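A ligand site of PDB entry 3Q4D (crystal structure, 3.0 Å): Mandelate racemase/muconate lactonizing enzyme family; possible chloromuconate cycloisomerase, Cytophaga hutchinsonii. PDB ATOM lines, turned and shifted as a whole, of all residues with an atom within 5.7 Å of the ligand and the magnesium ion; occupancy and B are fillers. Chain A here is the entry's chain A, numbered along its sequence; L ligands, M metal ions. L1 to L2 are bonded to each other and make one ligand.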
ATOM      1  N   PHE A  19      13.351   2.559   1.833  1.00  0.00           N
ATOM      2  CA  PHE A  19      12.880   1.739   0.739  1.00  0.00           C
ATOM      3  C   PHE A  19      14.069   1.056   0.098  1.00  0.00           C
ATOM      4  O   PHE A  19      15.067   1.710  -0.194  1.00  0.00           O
ATOM      5  CB  PHE A  19      12.174   2.640  -0.283  1.00  0.00           C
ATOM      6  CG  PHE A  19      11.532   1.916  -1.430  1.00  0.00           C
ATOM      7  CD1 PHE A  19      10.382   1.176  -1.241  1.00  0.00           C
ATOM      8  CD2 PHE A  19      12.036   2.028  -2.708  1.00  0.00           C
ATOM      9  CE1 PHE A  19       9.765   0.535  -2.317  1.00  0.00           C
ATOM     10  CE2 PHE A  19      11.429   1.406  -3.778  1.00  0.00           C
ATOM     11  CZ  PHE A  19      10.295   0.651  -3.582  1.00  0.00           C
ATOM     12  N   ILE A  21      15.553  -1.828  -2.712  1.00  0.00           N
ATOM     13  CA  ILE A  21      15.466  -2.716  -3.863  1.00  0.00           C
ATOM     14  C   ILE A  21      16.856  -3.261  -4.171  1.00  0.00           C
ATOM     15  O   ILE A  21      17.832  -2.809  -3.607  1.00  0.00           O
ATOM     16  CB  ILE A  21      14.894  -2.001  -5.108  1.00  0.00           C
ATOM     17  CG1 ILE A  21      15.753  -0.787  -5.466  1.00  0.00           C
ATOM     18  CG2 ILE A  21      13.491  -1.584  -4.881  1.00  0.00           C
ATOM     19  CD1 ILE A  21      15.326  -0.111  -6.739  1.00  0.00           C
ATOM     20  N   PHE A  51      14.820   8.474  -9.908  1.00  0.00           N
ATOM     21  CA  PHE A  51      15.500   7.335  -9.337  1.00  0.00           C
ATOM     22  C   PHE A  51      16.849   7.179 -10.028  1.00  0.00           C
ATOM     23  O   PHE A  51      16.911   6.683 -11.133  1.00  0.00           O
ATOM     24  CB  PHE A  51      14.689   6.103  -9.637  1.00  0.00           C
ATOM     25  CG  PHE A  51      14.260   5.333  -8.446  1.00  0.00           C
ATOM     26  CD1 PHE A  51      14.895   4.149  -8.113  1.00  0.00           C
ATOM     27  CD2 PHE A  51      13.180   5.754  -7.687  1.00  0.00           C
ATOM     28  CE1 PHE A  51      14.466   3.401  -7.029  1.00  0.00           C
ATOM     29  CE2 PHE A  51      12.749   4.999  -6.595  1.00  0.00           C
ATOM     30  CZ  PHE A  51      13.401   3.830  -6.270  1.00  0.00           C
ATOM     31  N   ILE A  54      17.748   4.006 -12.169  1.00  0.00           N
ATOM     32  CA  ILE A  54      16.849   3.587 -13.236  1.00  0.00           C
ATOM     33  C   ILE A  54      16.596   4.670 -14.273  1.00  0.00           C
ATOM     34  O   ILE A  54      16.711   4.421 -15.482  1.00  0.00           O
ATOM     35  CB  ILE A  54      15.520   3.072 -12.691  1.00  0.00           C
ATOM     36  CG1 ILE A  54      15.765   1.937 -11.704  1.00  0.00           C
ATOM     37  CG2 ILE A  54      14.605   2.636 -13.835  1.00  0.00           C
ATOM     38  CD1 ILE A  54      14.502   1.312 -11.196  1.00  0.00           C
ATOM     39  N   ASP A 133      -1.138  -3.262  -4.619  1.00  0.00           N
ATOM     40  CA  ASP A 133      -0.364  -4.143  -3.794  1.00  0.00           C
ATOM     41  C   ASP A 133       0.320  -3.285  -2.761  1.00  0.00           C
ATOM     42  O   ASP A 133       0.101  -2.081  -2.711  1.00  0.00           O
ATOM     43  CB  ASP A 133       0.663  -4.885  -4.656  1.00  0.00           C
ATOM     44  CG  ASP A 133       1.551  -3.953  -5.486  1.00  0.00           C
ATOM     45  OD1 ASP A 133       1.784  -4.265  -6.657  1.00  0.00           O
ATOM     46  OD2 ASP A 133       2.033  -2.920  -4.963  1.00  0.00           O
ATOM     47  N   THR A 135       4.508  -3.058  -1.088  1.00  0.00           N
ATOM     48  CA  THR A 135       5.849  -3.555  -1.327  1.00  0.00           C
ATOM     49  C   THR A 135       6.611  -3.906  -0.061  1.00  0.00           C
ATOM     50  O   THR A 135       6.695  -3.115   0.875  1.00  0.00           O
ATOM     51  CB  THR A 135       6.672  -2.529  -2.148  1.00  0.00           C
ATOM     52  OG1 THR A 135       6.078  -2.360  -3.426  1.00  0.00           O
ATOM     53  CG2 THR A 135       8.091  -2.985  -2.363  1.00  0.00           C
ATOM     54  N   LYS A 160       3.756  -7.161  -3.021  1.00  0.00           N
ATOM     55  CA  LYS A 160       4.875  -7.117  -3.957  1.00  0.00           C
ATOM     56  C   LYS A 160       6.199  -7.276  -3.219  1.00  0.00           C
ATOM     57  O   LYS A 160       6.522  -6.483  -2.355  1.00  0.00           O
ATOM     58  CB  LYS A 160       4.850  -5.818  -4.760  1.00  0.00           C
ATOM     59  CG  LYS A 160       6.023  -5.619  -5.676  1.00  0.00           C
ATOM     60  CD  LYS A 160       5.713  -4.563  -6.715  1.00  0.00           C
ATOM     61  CE  LYS A 160       6.948  -4.133  -7.453  1.00  0.00           C
ATOM     62  NZ  LYS A 160       6.656  -3.093  -8.459  1.00  0.00           N
ATOM     63  N   LYS A 162      10.356  -7.548  -3.119  1.00  0.00           N
ATOM     64  CA  LYS A 162      11.589  -7.202  -3.809  1.00  0.00           C
ATOM     65  C   LYS A 162      12.638  -8.304  -3.625  1.00  0.00           C
ATOM     66  O   LYS A 162      13.115  -8.561  -2.523  1.00  0.00           O
ATOM     67  CB  LYS A 162      12.120  -5.848  -3.340  1.00  0.00           C
ATOM     68  CG  LYS A 162      11.243  -4.674  -3.708  1.00  0.00           C
ATOM     69  CD  LYS A 162      11.199  -4.475  -5.205  1.00  0.00           C
ATOM     70  CE  LYS A 162      10.486  -3.215  -5.578  1.00  0.00           C
ATOM     71  NZ  LYS A 162      10.584  -2.958  -7.043  1.00  0.00           N
ATOM     72  N   ASP A 190       9.742  -8.848  -7.763  1.00  0.00           N
ATOM     73  CA  ASP A 190      10.442  -7.848  -8.567  1.00  0.00           C
ATOM     74  C   ASP A 190      11.925  -7.894  -8.231  1.00  0.00           C
ATOM     75  O   ASP A 190      12.311  -7.628  -7.101  1.00  0.00           O
ATOM     76  CB  ASP A 190       9.861  -6.452  -8.281  1.00  0.00           C
ATOM     77  CG  ASP A 190      10.378  -5.383  -9.238  1.00  0.00           C
ATOM     78  OD1 ASP A 190      11.448  -5.577  -9.863  1.00  0.00           O
ATOM     79  OD2 ASP A 190       9.716  -4.347  -9.366  1.00  0.00           O
ATOM     80  N   ASN A 192      14.373  -6.204 -10.018  1.00  0.00           N
ATOM     81  CA  ASN A 192      15.077  -5.012 -10.476  1.00  0.00           C
ATOM     82  C   ASN A 192      16.426  -5.324 -11.087  1.00  0.00           C
ATOM     83  O   ASN A 192      17.433  -4.779 -10.651  1.00  0.00           O
ATOM     84  CB  ASN A 192      15.246  -3.992  -9.358  1.00  0.00           C
ATOM     85  CG  ASN A 192      13.944  -3.353  -8.963  1.00  0.00           C
ATOM     86  OD1 ASN A 192      13.329  -2.657  -9.765  1.00  0.00           O
ATOM     87  ND2 ASN A 192      13.501  -3.583  -7.730  1.00  0.00           N
ATOM     88  N   GLU A 216       8.852  -9.178 -12.031  1.00  0.00           N
ATOM     89  CA  GLU A 216       9.280  -8.016 -12.778  1.00  0.00           C
ATOM     90  C   GLU A 216      10.779  -8.024 -13.004  1.00  0.00           C
ATOM     91  O   GLU A 216      11.526  -8.350 -12.113  1.00  0.00           O
ATOM     92  CB  GLU A 216       8.906  -6.718 -12.066  1.00  0.00           C
ATOM     93  CG  GLU A 216       7.438  -6.361 -12.083  1.00  0.00           C
ATOM     94  CD  GLU A 216       7.146  -5.132 -11.224  1.00  0.00           C
ATOM     95  OE1 GLU A 216       7.859  -4.127 -11.376  1.00  0.00           O
ATOM     96  OE2 GLU A 216       6.193  -5.179 -10.402  1.00  0.00           O
ATOM     97  N   ASP A 241       9.892  -4.247 -16.821  1.00  0.00           N
ATOM     98  CA  ASP A 241       9.796  -2.928 -16.218  1.00  0.00           C
ATOM     99  C   ASP A 241      10.835  -2.001 -16.848  1.00  0.00           C
ATOM    100  O   ASP A 241      10.542  -1.337 -17.835  1.00  0.00           O
ATOM    101  CB  ASP A 241       9.980  -3.021 -14.717  1.00  0.00           C
ATOM    102  CG  ASP A 241       9.468  -1.807 -13.988  1.00  0.00           C
ATOM    103  OD1 ASP A 241       9.464  -0.717 -14.585  1.00  0.00           O
ATOM    104  OD2 ASP A 241       9.089  -1.942 -12.800  1.00  0.00           O
ATOM    105  N   GLU A 242      12.042  -1.973 -16.287  1.00  0.00           N
ATOM    106  CA  GLU A 242      13.117  -1.149 -16.845  1.00  0.00           C
ATOM    107  C   GLU A 242      13.320  -1.406 -18.353  1.00  0.00           C
ATOM    108  O   GLU A 242      13.701  -0.527 -19.096  1.00  0.00           O
ATOM    109  CB  GLU A 242      14.444  -1.372 -16.095  1.00  0.00           C
ATOM    110  CG  GLU A 242      14.455  -0.890 -14.642  1.00  0.00           C
ATOM    111  CD  GLU A 242      13.950  -1.924 -13.622  1.00  0.00           C
ATOM    112  OE1 GLU A 242      12.767  -2.331 -13.683  1.00  0.00           O
ATOM    113  OE2 GLU A 242      14.734  -2.307 -12.742  1.00  0.00           O
ATOM    114  N   ASN A 263       5.139  -3.498 -17.147  1.00  0.00           N
ATOM    115  CA  ASN A 263       4.935  -2.519 -16.110  1.00  0.00           C
ATOM    116  C   ASN A 263       5.091  -1.082 -16.656  1.00  0.00           C
ATOM    117  O   ASN A 263       6.194  -0.620 -16.977  1.00  0.00           O
ATOM    118  CB  ASN A 263       5.878  -2.770 -14.943  1.00  0.00           C
ATOM    119  CG  ASN A 263       5.546  -1.932 -13.728  1.00  0.00           C
ATOM    120  OD1 ASN A 263       4.924  -0.883 -13.846  1.00  0.00           O
ATOM    121  ND2 ASN A 263       5.968  -2.388 -12.563  1.00  0.00           N
ATOM    122  N   LYS A 265       4.982   2.941 -16.474  1.00  0.00           N
ATOM    123  CA  LYS A 265       5.188   4.057 -15.548  1.00  0.00           C
ATOM    124  C   LYS A 265       5.316   5.347 -16.337  1.00  0.00           C
ATOM    125  O   LYS A 265       6.080   5.396 -17.291  1.00  0.00           O
ATOM    126  CB  LYS A 265       6.469   3.859 -14.723  1.00  0.00           C
ATOM    127  CG  LYS A 265       6.555   2.585 -13.875  1.00  0.00           C
ATOM    128  CD  LYS A 265       7.806   2.621 -13.012  1.00  0.00           C
ATOM    129  CE  LYS A 265       8.255   1.270 -12.503  1.00  0.00           C
ATOM    130  NZ  LYS A 265       7.413   0.743 -11.384  1.00  0.00           N
ATOM    131  N   GLY A 292       2.479   1.283 -12.509  1.00  0.00           N
ATOM    132  CA  GLY A 292       3.236   1.561 -11.298  1.00  0.00           C
ATOM    133  C   GLY A 292       3.859   2.934 -11.226  1.00  0.00           C
ATOM    134  O   GLY A 292       3.323   3.896 -11.730  1.00  0.00           O
ATOM    135  N   GLY A 293       5.017   3.034 -10.602  1.00  0.00           N
ATOM    136  CA  GLY A 293       5.681   4.310 -10.437  1.00  0.00           C
ATOM    137  C   GLY A 293       6.890   4.225  -9.531  1.00  0.00           C
ATOM    138  O   GLY A 293       7.419   3.161  -9.264  1.00  0.00           O
ATOM    139  N   PHE A 294       7.350   5.355  -9.025  1.00  0.00           N
ATOM    140  CA  PHE A 294       8.506   5.326  -8.142  1.00  0.00           C
ATOM    141  C   PHE A 294       8.165   5.858  -6.763  1.00  0.00           C
ATOM    142  O   PHE A 294       7.379   5.259  -6.069  1.00  0.00           O
ATOM    143  CB  PHE A 294       9.718   6.012  -8.779  1.00  0.00           C
ATOM    144  CG  PHE A 294      10.181   5.338 -10.037  1.00  0.00           C
ATOM    145  CD1 PHE A 294      11.201   4.395 -10.009  1.00  0.00           C
ATOM    146  CD2 PHE A 294       9.592   5.622 -11.263  1.00  0.00           C
ATOM    147  CE1 PHE A 294      11.627   3.780 -11.142  1.00  0.00           C
ATOM    148  CE2 PHE A 294      10.004   5.005 -12.416  1.00  0.00           C
ATOM    149  CZ  PHE A 294      11.024   4.079 -12.359  1.00  0.00           C
ATOM    150  N   LEU A 295       8.735   6.980  -6.352  1.00  0.00           N
ATOM    151  CA  LEU A 295       8.353   7.562  -5.068  1.00  0.00           C
ATOM    152  C   LEU A 295       7.528   8.840  -5.197  1.00  0.00           C
ATOM    153  O   LEU A 295       7.545   9.687  -4.318  1.00  0.00           O
ATOM    154  CB  LEU A 295       9.583   7.780  -4.185  1.00  0.00           C
ATOM    155  CG  LEU A 295       9.974   6.637  -3.254  1.00  0.00           C
ATOM    156  CD1 LEU A 295       9.735   5.297  -3.877  1.00  0.00           C
ATOM    157  CD2 LEU A 295      11.413   6.746  -2.875  1.00  0.00           C
ATOM    158  N   PHE A 301       0.790   9.683  -8.420  1.00  0.00           N
ATOM    159  CA  PHE A 301       0.044   8.461  -8.562  1.00  0.00           C
ATOM    160  C   PHE A 301      -1.404   8.701  -8.931  1.00  0.00           C
ATOM    161  O   PHE A 301      -2.093   7.815  -9.432  1.00  0.00           O
ATOM    162  CB  PHE A 301       0.160   7.604  -7.308  1.00  0.00           C
ATOM    163  CG  PHE A 301       1.406   6.781  -7.262  1.00  0.00           C
ATOM    164  CD1 PHE A 301       1.469   5.563  -7.909  1.00  0.00           C
ATOM    165  CD2 PHE A 301       2.503   7.224  -6.567  1.00  0.00           C
ATOM    166  CE1 PHE A 301       2.631   4.819  -7.860  1.00  0.00           C
ATOM    167  CE2 PHE A 301       3.660   6.467  -6.504  1.00  0.00           C
ATOM    168  CZ  PHE A 301       3.722   5.274  -7.158  1.00  0.00           C
ATOM    169  N   ASP A 318       0.403  -0.960  -8.823  1.00  0.00           N
ATOM    170  CA  ASP A 318       1.430  -0.799  -7.796  1.00  0.00           C
ATOM    171  C   ASP A 318       1.466   0.680  -7.421  1.00  0.00           C
ATOM    172  O   ASP A 318       2.248   1.442  -7.940  1.00  0.00           O
ATOM    173  CB  ASP A 318       2.793  -1.257  -8.340  1.00  0.00           C
ATOM    174  CG  ASP A 318       3.890  -1.184  -7.314  1.00  0.00           C
ATOM    175  OD1 ASP A 318       5.027  -0.825  -7.689  1.00  0.00           O
ATOM    176  OD2 ASP A 318       3.642  -1.484  -6.134  1.00  0.00           O
ATOM    177  N   PHE A 319       0.579   1.082  -6.530  1.00  0.00           N
ATOM    178  CA  PHE A 319       0.457   2.494  -6.185  1.00  0.00           C
ATOM    179  C   PHE A 319       0.717   2.725  -4.711  1.00  0.00           C
ATOM    180  O   PHE A 319      -0.019   3.473  -4.080  1.00  0.00           O
ATOM    181  CB  PHE A 319      -0.950   2.991  -6.488  1.00  0.00           C
ATOM    182  CG  PHE A 319      -1.274   3.042  -7.949  1.00  0.00           C
ATOM    183  CD1 PHE A 319      -0.297   2.910  -8.912  1.00  0.00           C
ATOM    184  CD2 PHE A 319      -2.586   3.248  -8.360  1.00  0.00           C
ATOM    185  CE1 PHE A 319      -0.622   2.956 -10.253  1.00  0.00           C
ATOM    186  CE2 PHE A 319      -2.914   3.311  -9.700  1.00  0.00           C
ATOM    187  CZ  PHE A 319      -1.936   3.156 -10.643  1.00  0.00           C
ATOM    188  N   ASP A 320       1.740   2.096  -4.157  1.00  0.00           N
ATOM    189  CA  ASP A 320       1.859   1.970  -2.708  1.00  0.00           C
ATOM    190  C   ASP A 320       2.716   3.030  -2.019  1.00  0.00           C
ATOM    191  O   ASP A 320       2.414   3.444  -0.917  1.00  0.00           O
ATOM    192  CB  ASP A 320       2.326   0.569  -2.337  1.00  0.00           C
ATOM    193  CG  ASP A 320       3.740   0.268  -2.790  1.00  0.00           C
ATOM    194  OD1 ASP A 320       4.190   0.818  -3.824  1.00  0.00           O
ATOM    195  OD2 ASP A 320       4.417  -0.531  -2.103  1.00  0.00           O
ATOM    196  N   THR A 321       3.765   3.473  -2.683  1.00  0.00           N
ATOM    197  CA  THR A 321       4.772   4.295  -2.035  1.00  0.00           C
ATOM    198  C   THR A 321       4.309   5.565  -1.294  1.00  0.00           C
ATOM    199  O   THR A 321       4.943   5.968  -0.346  1.00  0.00           O
ATOM    200  CB  THR A 321       5.892   4.675  -3.012  1.00  0.00           C
ATOM    201  OG1 THR A 321       5.326   5.081  -4.258  1.00  0.00           O
ATOM    202  CG2 THR A 321       6.772   3.497  -3.248  1.00  0.00           C
HETATM  203  N1  LIG L   1       6.062  -0.192  -5.415  1.00  0.00           N
HETATM  204  C1  LIG L   1       6.923   0.934  -5.783  1.00  0.00           C
HETATM  205  C2  LIG L   1       6.135   1.957  -6.539  1.00  0.00           C
HETATM  206  C3  LIG L   1       8.098   0.444  -6.588  1.00  0.00           C
HETATM  207  O1  LIG L   1       8.625  -0.620  -6.349  1.00  0.00           O
HETATM  208  N1  LG2 L   2       8.554   1.267  -7.538  1.00  0.00           N
HETATM  209  C1  LG2 L   2       9.668   0.922  -8.441  1.00  0.00           C
HETATM  210  C2  LG2 L   2       9.343  -0.415  -9.049  1.00  0.00           C
HETATM  211  O1  LG2 L   2       8.216  -0.705  -9.447  1.00  0.00           O
HETATM  212  C3  LG2 L   2      11.019   0.892  -7.716  1.00  0.00           C
HETATM  213  O2  LG2 L   2      10.217  -1.266  -9.141  1.00  0.00           O
HETATM  214 MG    MG M   1       9.524  -2.707 -11.019  1.00  0.00          MG
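An oxygen (O1) of LG2 L2 lies within salt-bridge range of the side-chain amino group (NZ) of Lys 265, 2.5 Å away. OD1 of Asp 318 lies within salt-bridge range of N1 of LIG L1 (2.6 Å). OD1 of Asp 320 lies within salt-bridge range of N1 of LIG L1. An oxygen (O1) of LIG L1 lies within hydrogen-bond range of the side-chain amino group (NZ) of Lys 162. The backbone carbonyl oxygen (O) of Gly 293 lies within hydrogen-bond range of a nitrogen (N1) of LG2 L2, 2.8 Å away. OG1 of Thr 135 is in hydrogen-bond range of N1 of LIG L1. An oxygen (O1) of LG2 L2 is in salt-bridge range of the side-chain amino group (NZ) of Lys 160 (3.0 Å). The side-chain amide oxygen of Asn 192 lies close to an oxygen (O2) of LG2 L2.
The side-chain carboxylate of Asp 241 lies close to the side-chain amino group of Lys 265. The side-chain amide nitrogen (ND2) of Asn 263 lies close to the side-chain carboxylate (OD2) of Asp 241, 3.2 Å away. The side-chain carboxylate (OD2) of Asp 190 sits close to the side-chain amino group (NZ) of Lys 160, 3.4 Å away. The side-chain carboxylate of Asp 190 lies within hydrogen-bond range of the backbone NH of Asn 192 (3.0 Å). OD2 of Asp 318 sits close to OD2 of Asp 133 (2.5 Å). The side-chain amino group of Lys 162 lies close to the side-chain amide nitrogen of Asn 192, at 3.1 Å. The side-chain amide oxygen (OD1) of Asn 192 sits close to the side-chain carboxylate (OE2) of Glu 242 (3.3 Å). OG1 of Thr 321 lies within hydrogen-bond range of O of Phe 294.
CZ of Phe 19 touches O1 of LIG L1 (3.5 Å). Phe 294 touches the ligand. Thr 321 touches the ligand. Hydrophobic or aromatic side chains that line the ligand: Phe 19. Within 4 Å of the ligand: Phe 19, Thr 135, Lys 160, Lys 162, Asp 190, Asn 192, Glu 216, Asp 241, Lys 265, Gly 293, Phe 294, Asp 318, Asp 320 and Thr 321.
NZ of Lys 160 touches the magnesium ion, 3.9 Å away. Asn 263 touches the magnesium ion. Within 4 Å of the magnesium ion: Lys 160, Asp 190, Glu 216, Asp 241 and Asn 263.
The magnesium ion is bound by the side-chain carboxylate of Asp 241, the side-chain carboxylate of Glu 216, the side-chain carboxylate of Asp 190 and an oxygen (O2) of LG2 L2. The magnesium ion has four donor atoms within binding distance.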
